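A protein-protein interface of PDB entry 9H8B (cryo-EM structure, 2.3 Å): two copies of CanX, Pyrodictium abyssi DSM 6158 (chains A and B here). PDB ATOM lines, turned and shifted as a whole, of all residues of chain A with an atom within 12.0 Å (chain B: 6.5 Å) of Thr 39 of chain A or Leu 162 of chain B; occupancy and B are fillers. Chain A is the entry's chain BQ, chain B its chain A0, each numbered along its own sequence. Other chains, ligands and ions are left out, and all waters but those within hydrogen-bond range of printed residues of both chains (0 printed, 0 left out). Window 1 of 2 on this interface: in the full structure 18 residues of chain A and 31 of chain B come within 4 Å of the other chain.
Of the 17 printed residues of chain B, 11 touch a printed residue of chain A. Printed residues of chain B that touch a printed residue of chain A: Leu 53, Asn 55, Thr 56, Ile 57, Ala 58, Phe 159, Asp 160, Ser 161, Leu 162, Pro 163 and Val 164. Of the 9 printed residues of chain A, 8 touch a printed residue of chain B. Printed residues of chain A that touch a printed residue of chain B: Ala 36, Thr 37, Gly 38, Thr 39, Ala 40, Gln 41, Ala 42 and Val 43. Hydrophobic or aromatic side chains of chain A that line the printed part of chain B: Ala 40 and Val 43. Among the printed residues, 20 pairs touch across the chains.
The side-chain amide nitrogen (ND2) of Asn 91 of chain B sits at hydrogen-bond distance from the backbone carbonyl oxygen (O) of Pro 163 of chain B (2.9 Å). The side-chain carboxylate (OD2) of Asp 160 of chain B sits close to the side-chain hydroxyl (OG) of Ser 161 of chain B (3.2 Å). The backbone carbonyl oxygen (O) of Met 69 of chain B lies close to the backbone NH (N) of Asn 55 of chain B.
Of the printed residues of chain B, Gly 38 of chain A touches Pro 163 (3.2 Å) and Val 164 (2.7 Å). Of chain B, only Asn 55, Thr 56, Ile 57 and Leu 162 come within 4 Å of Thr 39 of chain A. Of the printed residues of chain B, Gln 41 of chain A touches Ile 57 (2.9 Å), Ala 58 (3.3 Å), Phe 159 (3.8 Å) and Asp 160 (3.9 Å). Printed residues of chain B within 4 Å of Ala 42 of chain A: Phe 159. Printed residues of chain B within 4 Å of Val 43 of chain A: Phe 159 and Asp 160. Printed residues of chain A within 4 Å of Asn 55 of chain B: Thr 39. Thr 56 of chain B touches just these residues of chain A: Thr 39 (3.5 Å) and Ala 40 (3.7 Å). Met 69 of chain B touches none of the printed residues of chain A. No residue of chain A comes within 4 Å of Leu 95 of chain B. Phe 159 of chain B touches three residues of chain A. Of chain A, only Gln 41 (3.9 Å) and Val 43 (3.9 Å) come within 4 Å of Asp 160 of chain B. Of the printed residues of chain A, Ser 161 of chain B touches Ala 40. Leu 162 of chain B touches just these residues of chain A: Thr 39 (3.3 Å) and Ala 40 (3.0 Å). Pro 163 of chain B touches just one residue of chain A: Gly 38. Val 164 of chain B touches just these residues of chain A: Ala 36 (3.7 Å), Thr 37 (3.1 Å) and Gly 38 (2.7 Å). The nearest residue of chain B that does not touch Thr 39 of chain A is Met 69 of chain B (4.2 Å). The nearest residue of chain A that does not touch Leu 162 of chain B is Gly 38 of chain A (4.1 Å). The nearest printed residue of chain B that does not touch Ala 36 of chain A is Leu 53 of chain B (4.1 Å).
No position is printed for both chains.
Among the printed residues, merely in contact across the chains: Ala 36 of chain A with Val 164 of chain B (3.7 Å), Thr 37 of chain A with Leu 53 of chain B (3.6 Å), Thr 37 of chain A with Val 164 of chain B (3.1 Å), Gly 38 of chain A with Pro 163 of chain B (3.2 Å), Thr 39 of chain A with Asn 55 of chain B (3.96 Å), Thr 39 of chain A with Thr 56 of chain B (3.5 Å), Thr 39 of chain A with Leu 162 of chain B (3.3 Å), Ala 40 of chain A with Thr 56 of chain B (3.7 Å), Ala 40 of chain A with Ile 57 of chain B (3.3 Å), Ala 40 of chain A with Ser 161 of chain B (3.9 Å), Gln 41 of chain A with Ala 58 of chain B (3.3 Å), Gln 41 of chain A with Phe 159 of chain B (3.8 Å), Gln 41 of chain A with Asp 160 of chain B (3.9 Å), Val 43 of chain A with Phe 159 of chain B (3.3 Å) and Val 43 of chain A with Asp 160 of chain B (3.9 Å).
O of Val 164 of chain B lies within hydrogen-bond range of N of Gly 38 of chain A (2.7 Å). The backbone NH (N) of Ile 57 of chain B sits at hydrogen-bond distance from the backbone carbonyl oxygen (O) of Thr 39 of chain A, at 3.4 Å. The backbone NH (N) of Ala 40 of chain A is in hydrogen-bond range of the backbone carbonyl oxygen (O) of Leu 162 of chain B, 3.0 Å away. O of Ala 42 of chain A is in hydrogen-bond range of N of Phe 159 of chain B (2.9 Å). The backbone carbonyl oxygen (O) of Ile 57 of chain B is in hydrogen-bond range of the backbone NH (N) of Gln 41 of chain A (2.9 Å).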
ATOM      1  N   TYR A  35      33.120  -2.507 -21.307  1.00  0.00           N
ATOM      2  CA  TYR A  35      31.745  -2.307 -20.869  1.00  0.00           C
ATOM      3  C   TYR A  35      31.061  -3.650 -20.649  1.00  0.00           C
ATOM      4  O   TYR A  35      31.483  -4.684 -21.174  1.00  0.00           O
ATOM      5  CB  TYR A  35      30.947  -1.475 -21.881  1.00  0.00           C
ATOM      6  CG  TYR A  35      31.301  -0.005 -21.894  1.00  0.00           C
ATOM      7  CD1 TYR A  35      30.637   0.894 -21.070  1.00  0.00           C
ATOM      8  CD2 TYR A  35      32.289   0.487 -22.737  1.00  0.00           C
ATOM      9  CE1 TYR A  35      30.952   2.239 -21.077  1.00  0.00           C
ATOM     10  CE2 TYR A  35      32.612   1.831 -22.751  1.00  0.00           C
ATOM     11  CZ  TYR A  35      31.940   2.702 -21.920  1.00  0.00           C
ATOM     12  OH  TYR A  35      32.255   4.042 -21.931  1.00  0.00           O
ATOM     13  N   ALA A  36      29.991  -3.611 -19.856  1.00  0.00           N
ATOM     14  CA  ALA A  36      29.117  -4.755 -19.627  1.00  0.00           C
ATOM     15  C   ALA A  36      27.706  -4.227 -19.405  1.00  0.00           C
ATOM     16  O   ALA A  36      27.528  -3.169 -18.796  1.00  0.00           O
ATOM     17  CB  ALA A  36      29.577  -5.591 -18.428  1.00  0.00           C
ATOM     18  N   THR A  37      26.710  -4.964 -19.897  1.00  0.00           N
ATOM     19  CA  THR A  37      25.345  -4.458 -19.960  1.00  0.00           C
ATOM     20  C   THR A  37      24.354  -5.482 -19.421  1.00  0.00           C
ATOM     21  O   THR A  37      24.488  -6.684 -19.671  1.00  0.00           O
ATOM     22  CB  THR A  37      24.976  -4.078 -21.406  1.00  0.00           C
ATOM     23  OG1 THR A  37      25.881  -3.074 -21.880  1.00  0.00           O
ATOM     24  CG2 THR A  37      23.555  -3.537 -21.485  1.00  0.00           C
ATOM     25  N   GLY A  38      23.360  -4.994 -18.678  1.00  0.00           N
ATOM     26  CA  GLY A  38      22.235  -5.801 -18.238  1.00  0.00           C
ATOM     27  C   GLY A  38      20.912  -5.124 -18.542  1.00  0.00           C
ATOM     28  O   GLY A  38      20.891  -4.087 -19.210  1.00  0.00           O
ATOM     29  N   THR A  39      19.804  -5.681 -18.052  1.00  0.00           N
ATOM     30  CA  THR A  39      18.480  -5.136 -18.336  1.00  0.00           C
ATOM     31  C   THR A  39      17.578  -5.315 -17.122  1.00  0.00           C
ATOM     32  O   THR A  39      17.850  -6.125 -16.233  1.00  0.00           O
ATOM     33  CB  THR A  39      17.830  -5.801 -19.561  1.00  0.00           C
ATOM     34  OG1 THR A  39      17.953  -7.226 -19.462  1.00  0.00           O
ATOM     35  CG2 THR A  39      18.468  -5.318 -20.858  1.00  0.00           C
ATOM     36  N   ALA A  40      16.496  -4.538 -17.100  1.00  0.00           N
ATOM     37  CA  ALA A  40      15.492  -4.622 -16.047  1.00  0.00           C
ATOM     38  C   ALA A  40      14.151  -4.164 -16.605  1.00  0.00           C
ATOM     39  O   ALA A  40      14.088  -3.468 -17.622  1.00  0.00           O
ATOM     40  CB  ALA A  40      15.883  -3.783 -14.825  1.00  0.00           C
ATOM     41  N   GLN A  41      13.075  -4.560 -15.926  1.00  0.00           N
ATOM     42  CA  GLN A  41      11.733  -4.223 -16.384  1.00  0.00           C
ATOM     43  C   GLN A  41      10.739  -4.383 -15.241  1.00  0.00           C
ATOM     44  O   GLN A  41      11.028  -5.018 -14.222  1.00  0.00           O
ATOM     45  CB  GLN A  41      11.310  -5.093 -17.571  1.00  0.00           C
ATOM     46  CG  GLN A  41      11.220  -6.575 -17.243  1.00  0.00           C
ATOM     47  CD  GLN A  41      10.462  -7.361 -18.293  1.00  0.00           C
ATOM     48  OE1 GLN A  41       9.544  -8.117 -17.976  1.00  0.00           O
ATOM     49  NE2 GLN A  41      10.843  -7.187 -19.553  1.00  0.00           N
ATOM     50  N   ALA A  42       9.560  -3.788 -15.431  1.00  0.00           N
ATOM     51  CA  ALA A  42       8.437  -3.948 -14.506  1.00  0.00           C
ATOM     52  C   ALA A  42       7.167  -3.618 -15.281  1.00  0.00           C
ATOM     53  O   ALA A  42       6.937  -2.451 -15.611  1.00  0.00           O
ATOM     54  CB  ALA A  42       8.595  -3.045 -13.288  1.00  0.00           C
ATOM     55  N   VAL A  43       6.353  -4.633 -15.570  1.00  0.00           N
ATOM     56  CA  VAL A  43       5.257  -4.481 -16.518  1.00  0.00           C
ATOM     57  C   VAL A  43       3.918  -4.948 -15.943  1.00  0.00           C
ATOM     58  O   VAL A  43       3.032  -5.340 -16.695  1.00  0.00           O
ATOM     59  CB  VAL A  43       5.569  -5.207 -17.841  1.00  0.00           C
ATOM     60  CG1 VAL A  43       6.744  -4.548 -18.549  1.00  0.00           C
ATOM     61  CG2 VAL A  43       5.858  -6.680 -17.581  1.00  0.00           C
ATOM     62  N   LEU B  53      26.205 -11.159 -18.570  1.00  0.00           N
ATOM     63  CA  LEU B  53      25.091 -10.745 -17.715  1.00  0.00           C
ATOM     64  C   LEU B  53      23.792 -11.005 -18.468  1.00  0.00           C
ATOM     65  O   LEU B  53      23.329 -10.179 -19.256  1.00  0.00           O
ATOM     66  CB  LEU B  53      25.234  -9.281 -17.316  1.00  0.00           C
ATOM     67  CG  LEU B  53      26.536  -8.899 -16.610  1.00  0.00           C
ATOM     68  CD1 LEU B  53      26.588  -7.403 -16.347  1.00  0.00           C
ATOM     69  CD2 LEU B  53      26.691  -9.681 -15.316  1.00  0.00           C
ATOM     70  N   ASN B  55      20.620 -12.048 -17.028  1.00  0.00           N
ATOM     71  CA  ASN B  55      19.445 -12.128 -16.171  1.00  0.00           C
ATOM     72  C   ASN B  55      18.819 -10.747 -16.050  1.00  0.00           C
ATOM     73  O   ASN B  55      19.506  -9.725 -16.132  1.00  0.00           O
ATOM     74  CB  ASN B  55      19.783 -12.676 -14.780  1.00  0.00           C
ATOM     75  CG  ASN B  55      19.484 -14.157 -14.649  1.00  0.00           C
ATOM     76  OD1 ASN B  55      20.253 -15.000 -15.111  1.00  0.00           O
ATOM     77  ND2 ASN B  55      18.362 -14.481 -14.017  1.00  0.00           N
ATOM     78  N   THR B  56      17.505 -10.725 -15.852  1.00  0.00           N
ATOM     79  CA  THR B  56      16.729  -9.494 -15.843  1.00  0.00           C
ATOM     80  C   THR B  56      16.119  -9.268 -14.467  1.00  0.00           C
ATOM     81  O   THR B  56      15.506 -10.178 -13.898  1.00  0.00           O
ATOM     82  CB  THR B  56      15.626  -9.539 -16.904  1.00  0.00           C
ATOM     83  OG1 THR B  56      16.179  -9.967 -18.154  1.00  0.00           O
ATOM     84  CG2 THR B  56      14.997  -8.165 -17.079  1.00  0.00           C
ATOM     85  N   ILE B  57      16.289  -8.060 -13.939  1.00  0.00           N
ATOM     86  CA  ILE B  57      15.608  -7.647 -12.717  1.00  0.00           C
ATOM     87  C   ILE B  57      14.169  -7.313 -13.090  1.00  0.00           C
ATOM     88  O   ILE B  57      13.895  -6.256 -13.663  1.00  0.00           O
ATOM     89  CB  ILE B  57      16.304  -6.450 -12.059  1.00  0.00           C
ATOM     90  CG1 ILE B  57      17.732  -6.817 -11.650  1.00  0.00           C
ATOM     91  CG2 ILE B  57      15.512  -5.968 -10.852  1.00  0.00           C
ATOM     92  CD1 ILE B  57      18.622  -5.617 -11.401  1.00  0.00           C
ATOM     93  N   ALA B  58      13.241  -8.212 -12.767  1.00  0.00           N
ATOM     94  CA  ALA B  58      11.840  -8.082 -13.164  1.00  0.00           C
ATOM     95  C   ALA B  58      10.933  -8.238 -11.950  1.00  0.00           C
ATOM     96  O   ALA B  58      10.290  -9.279 -11.765  1.00  0.00           O
ATOM     97  CB  ALA B  58      11.485  -9.104 -14.244  1.00  0.00           C
ATOM     98  N   MET B  69      22.519 -11.756 -11.320  1.00  0.00           N
ATOM     99  CA  MET B  69      22.550 -11.299 -12.707  1.00  0.00           C
ATOM    100  C   MET B  69      23.364 -12.198 -13.632  1.00  0.00           C
ATOM    101  O   MET B  69      22.875 -12.602 -14.690  1.00  0.00           O
ATOM    102  CB  MET B  69      23.098  -9.868 -12.761  1.00  0.00           C
ATOM    103  CG  MET B  69      22.188  -8.839 -12.111  1.00  0.00           C
ATOM    104  SD  MET B  69      22.439  -7.174 -12.752  1.00  0.00           S
ATOM    105  CE  MET B  69      21.415  -7.222 -14.220  1.00  0.00           C
ATOM    106  N   ASN B  91      25.541   4.784 -16.197  1.00  0.00           N
ATOM    107  CA  ASN B  91      24.250   5.427 -16.414  1.00  0.00           C
ATOM    108  C   ASN B  91      23.441   5.516 -15.125  1.00  0.00           C
ATOM    109  O   ASN B  91      22.236   5.242 -15.118  1.00  0.00           O
ATOM    110  CB  ASN B  91      23.466   4.680 -17.498  1.00  0.00           C
ATOM    111  CG  ASN B  91      23.168   3.243 -17.117  1.00  0.00           C
ATOM    112  OD1 ASN B  91      23.919   2.618 -16.369  1.00  0.00           O
ATOM    113  ND2 ASN B  91      22.069   2.709 -17.636  1.00  0.00           N
ATOM    114  N   GLN B  94      20.444   8.069 -15.278  1.00  0.00           N
ATOM    115  CA  GLN B  94      19.233   7.614 -15.954  1.00  0.00           C
ATOM    116  C   GLN B  94      18.394   6.706 -15.060  1.00  0.00           C
ATOM    117  O   GLN B  94      17.161   6.735 -15.133  1.00  0.00           O
ATOM    118  CB  GLN B  94      19.604   6.895 -17.252  1.00  0.00           C
ATOM    119  CG  GLN B  94      18.437   6.249 -17.981  1.00  0.00           C
ATOM    120  CD  GLN B  94      18.869   5.525 -19.241  1.00  0.00           C
ATOM    121  OE1 GLN B  94      19.926   4.893 -19.276  1.00  0.00           O
ATOM    122  NE2 GLN B  94      18.052   5.612 -20.284  1.00  0.00           N
ATOM    123  N   LEU B  95      19.039   5.908 -14.209  1.00  0.00           N
ATOM    124  CA  LEU B  95      18.337   4.950 -13.364  1.00  0.00           C
ATOM    125  C   LEU B  95      17.740   5.573 -12.108  1.00  0.00           C
ATOM    126  O   LEU B  95      16.965   4.903 -11.417  1.00  0.00           O
ATOM    127  CB  LEU B  95      19.285   3.815 -12.965  1.00  0.00           C
ATOM    128  CG  LEU B  95      19.807   2.928 -14.098  1.00  0.00           C
ATOM    129  CD1 LEU B  95      21.029   2.145 -13.643  1.00  0.00           C
ATOM    130  CD2 LEU B  95      18.719   1.988 -14.592  1.00  0.00           C
ATOM    131  N   TYR B  98      13.805   5.698 -11.549  1.00  0.00           N
ATOM    132  CA  TYR B  98      13.136   4.405 -11.544  1.00  0.00           C
ATOM    133  C   TYR B  98      13.327   3.614 -10.256  1.00  0.00           C
ATOM    134  O   TYR B  98      12.623   2.620 -10.055  1.00  0.00           O
ATOM    135  CB  TYR B  98      13.630   3.550 -12.719  1.00  0.00           C
ATOM    136  CG  TYR B  98      13.303   4.119 -14.081  1.00  0.00           C
ATOM    137  CD1 TYR B  98      14.173   4.994 -14.717  1.00  0.00           C
ATOM    138  CD2 TYR B  98      12.126   3.777 -14.732  1.00  0.00           C
ATOM    139  CE1 TYR B  98      13.879   5.515 -15.963  1.00  0.00           C
ATOM    140  CE2 TYR B  98      11.822   4.291 -15.977  1.00  0.00           C
ATOM    141  CZ  TYR B  98      12.702   5.159 -16.589  1.00  0.00           C
ATOM    142  OH  TYR B  98      12.402   5.674 -17.828  1.00  0.00           O
ATOM    143  N   PHE B  99      14.248   4.020  -9.384  1.00  0.00           N
ATOM    144  CA  PHE B  99      14.579   3.244  -8.199  1.00  0.00           C
ATOM    145  C   PHE B  99      14.731   4.154  -6.989  1.00  0.00           C
ATOM    146  O   PHE B  99      15.246   5.270  -7.092  1.00  0.00           O
ATOM    147  CB  PHE B  99      15.877   2.450  -8.398  1.00  0.00           C
ATOM    148  CG  PHE B  99      15.710   1.207  -9.222  1.00  0.00           C
ATOM    149  CD1 PHE B  99      15.231   0.039  -8.655  1.00  0.00           C
ATOM    150  CD2 PHE B  99      16.040   1.206 -10.568  1.00  0.00           C
ATOM    151  CE1 PHE B  99      15.079  -1.106  -9.415  1.00  0.00           C
ATOM    152  CE2 PHE B  99      15.890   0.067 -11.333  1.00  0.00           C
ATOM    153  CZ  PHE B  99      15.410  -1.091 -10.755  1.00  0.00           C
ATOM    154  N   PHE B 159       7.645   0.138 -16.819  1.00  0.00           N
ATOM    155  CA  PHE B 159       8.623   0.352 -17.877  1.00  0.00           C
ATOM    156  C   PHE B 159       9.116  -1.003 -18.368  1.00  0.00           C
ATOM    157  O   PHE B 159       8.824  -2.045 -17.778  1.00  0.00           O
ATOM    158  CB  PHE B 159       9.792   1.214 -17.388  1.00  0.00           C
ATOM    159  CG  PHE B 159      10.485   0.662 -16.174  1.00  0.00           C
ATOM    160  CD1 PHE B 159      10.053   0.999 -14.902  1.00  0.00           C
ATOM    161  CD2 PHE B 159      11.568  -0.191 -16.303  1.00  0.00           C
ATOM    162  CE1 PHE B 159      10.687   0.493 -13.782  1.00  0.00           C
ATOM    163  CE2 PHE B 159      12.206  -0.700 -15.189  1.00  0.00           C
ATOM    164  CZ  PHE B 159      11.765  -0.357 -13.926  1.00  0.00           C
ATOM    165  N   ASP B 160       9.871  -0.969 -19.462  1.00  0.00           N
ATOM    166  CA  ASP B 160      10.475  -2.174 -20.015  1.00  0.00           C
ATOM    167  C   ASP B 160      11.663  -1.774 -20.876  1.00  0.00           C
ATOM    168  O   ASP B 160      11.765  -0.633 -21.335  1.00  0.00           O
ATOM    169  CB  ASP B 160       9.464  -2.986 -20.832  1.00  0.00           C
ATOM    170  CG  ASP B 160       9.003  -2.258 -22.080  1.00  0.00           C
ATOM    171  OD1 ASP B 160       8.118  -1.384 -21.967  1.00  0.00           O
ATOM    172  OD2 ASP B 160       9.527  -2.561 -23.173  1.00  0.00           O
ATOM    173  N   SER B 161      12.563  -2.738 -21.086  1.00  0.00           N
ATOM    174  CA  SER B 161      13.743  -2.559 -21.936  1.00  0.00           C
ATOM    175  C   SER B 161      14.615  -1.403 -21.444  1.00  0.00           C
ATOM    176  O   SER B 161      14.880  -0.439 -22.167  1.00  0.00           O
ATOM    177  CB  SER B 161      13.339  -2.359 -23.400  1.00  0.00           C
ATOM    178  OG  SER B 161      12.492  -3.405 -23.844  1.00  0.00           O
ATOM    179  N   LEU B 162      15.063  -1.505 -20.193  1.00  0.00           N
ATOM    180  CA  LEU B 162      15.936  -0.502 -19.596  1.00  0.00           C
ATOM    181  C   LEU B 162      17.304  -1.109 -19.330  1.00  0.00           C
ATOM    182  O   LEU B 162      17.402  -2.077 -18.561  1.00  0.00           O
ATOM    183  CB  LEU B 162      15.331   0.039 -18.302  1.00  0.00           C
ATOM    184  CG  LEU B 162      15.943   1.334 -17.768  1.00  0.00           C
ATOM    185  CD1 LEU B 162      15.614   2.501 -18.687  1.00  0.00           C
ATOM    186  CD2 LEU B 162      15.458   1.611 -16.353  1.00  0.00           C
ATOM    187  N   PRO B 163      18.374  -0.589 -19.926  1.00  0.00           N
ATOM    188  CA  PRO B 163      19.696  -1.197 -19.753  1.00  0.00           C
ATOM    189  C   PRO B 163      20.450  -0.677 -18.539  1.00  0.00           C
ATOM    190  O   PRO B 163      20.264   0.451 -18.081  1.00  0.00           O
ATOM    191  CB  PRO B 163      20.415  -0.800 -21.050  1.00  0.00           C
ATOM    192  CG  PRO B 163      19.829   0.534 -21.390  1.00  0.00           C
ATOM    193  CD  PRO B 163      18.405   0.542 -20.872  1.00  0.00           C
ATOM    194  N   VAL B 164      21.321  -1.541 -18.020  1.00  0.00           N
ATOM    195  CA  VAL B 164      22.242  -1.207 -16.938  1.00  0.00           C
ATOM    196  C   VAL B 164      23.657  -1.425 -17.454  1.00  0.00           C
ATOM    197  O   VAL B 164      23.971  -2.500 -17.977  1.00  0.00           O
ATOM    198  CB  VAL B 164      21.983  -2.055 -15.679  1.00  0.00           C
ATOM    199  CG1 VAL B 164      22.676  -1.437 -14.474  1.00  0.00           C
ATOM    200  CG2 VAL B 164      20.489  -2.194 -15.427  1.00  0.00           C
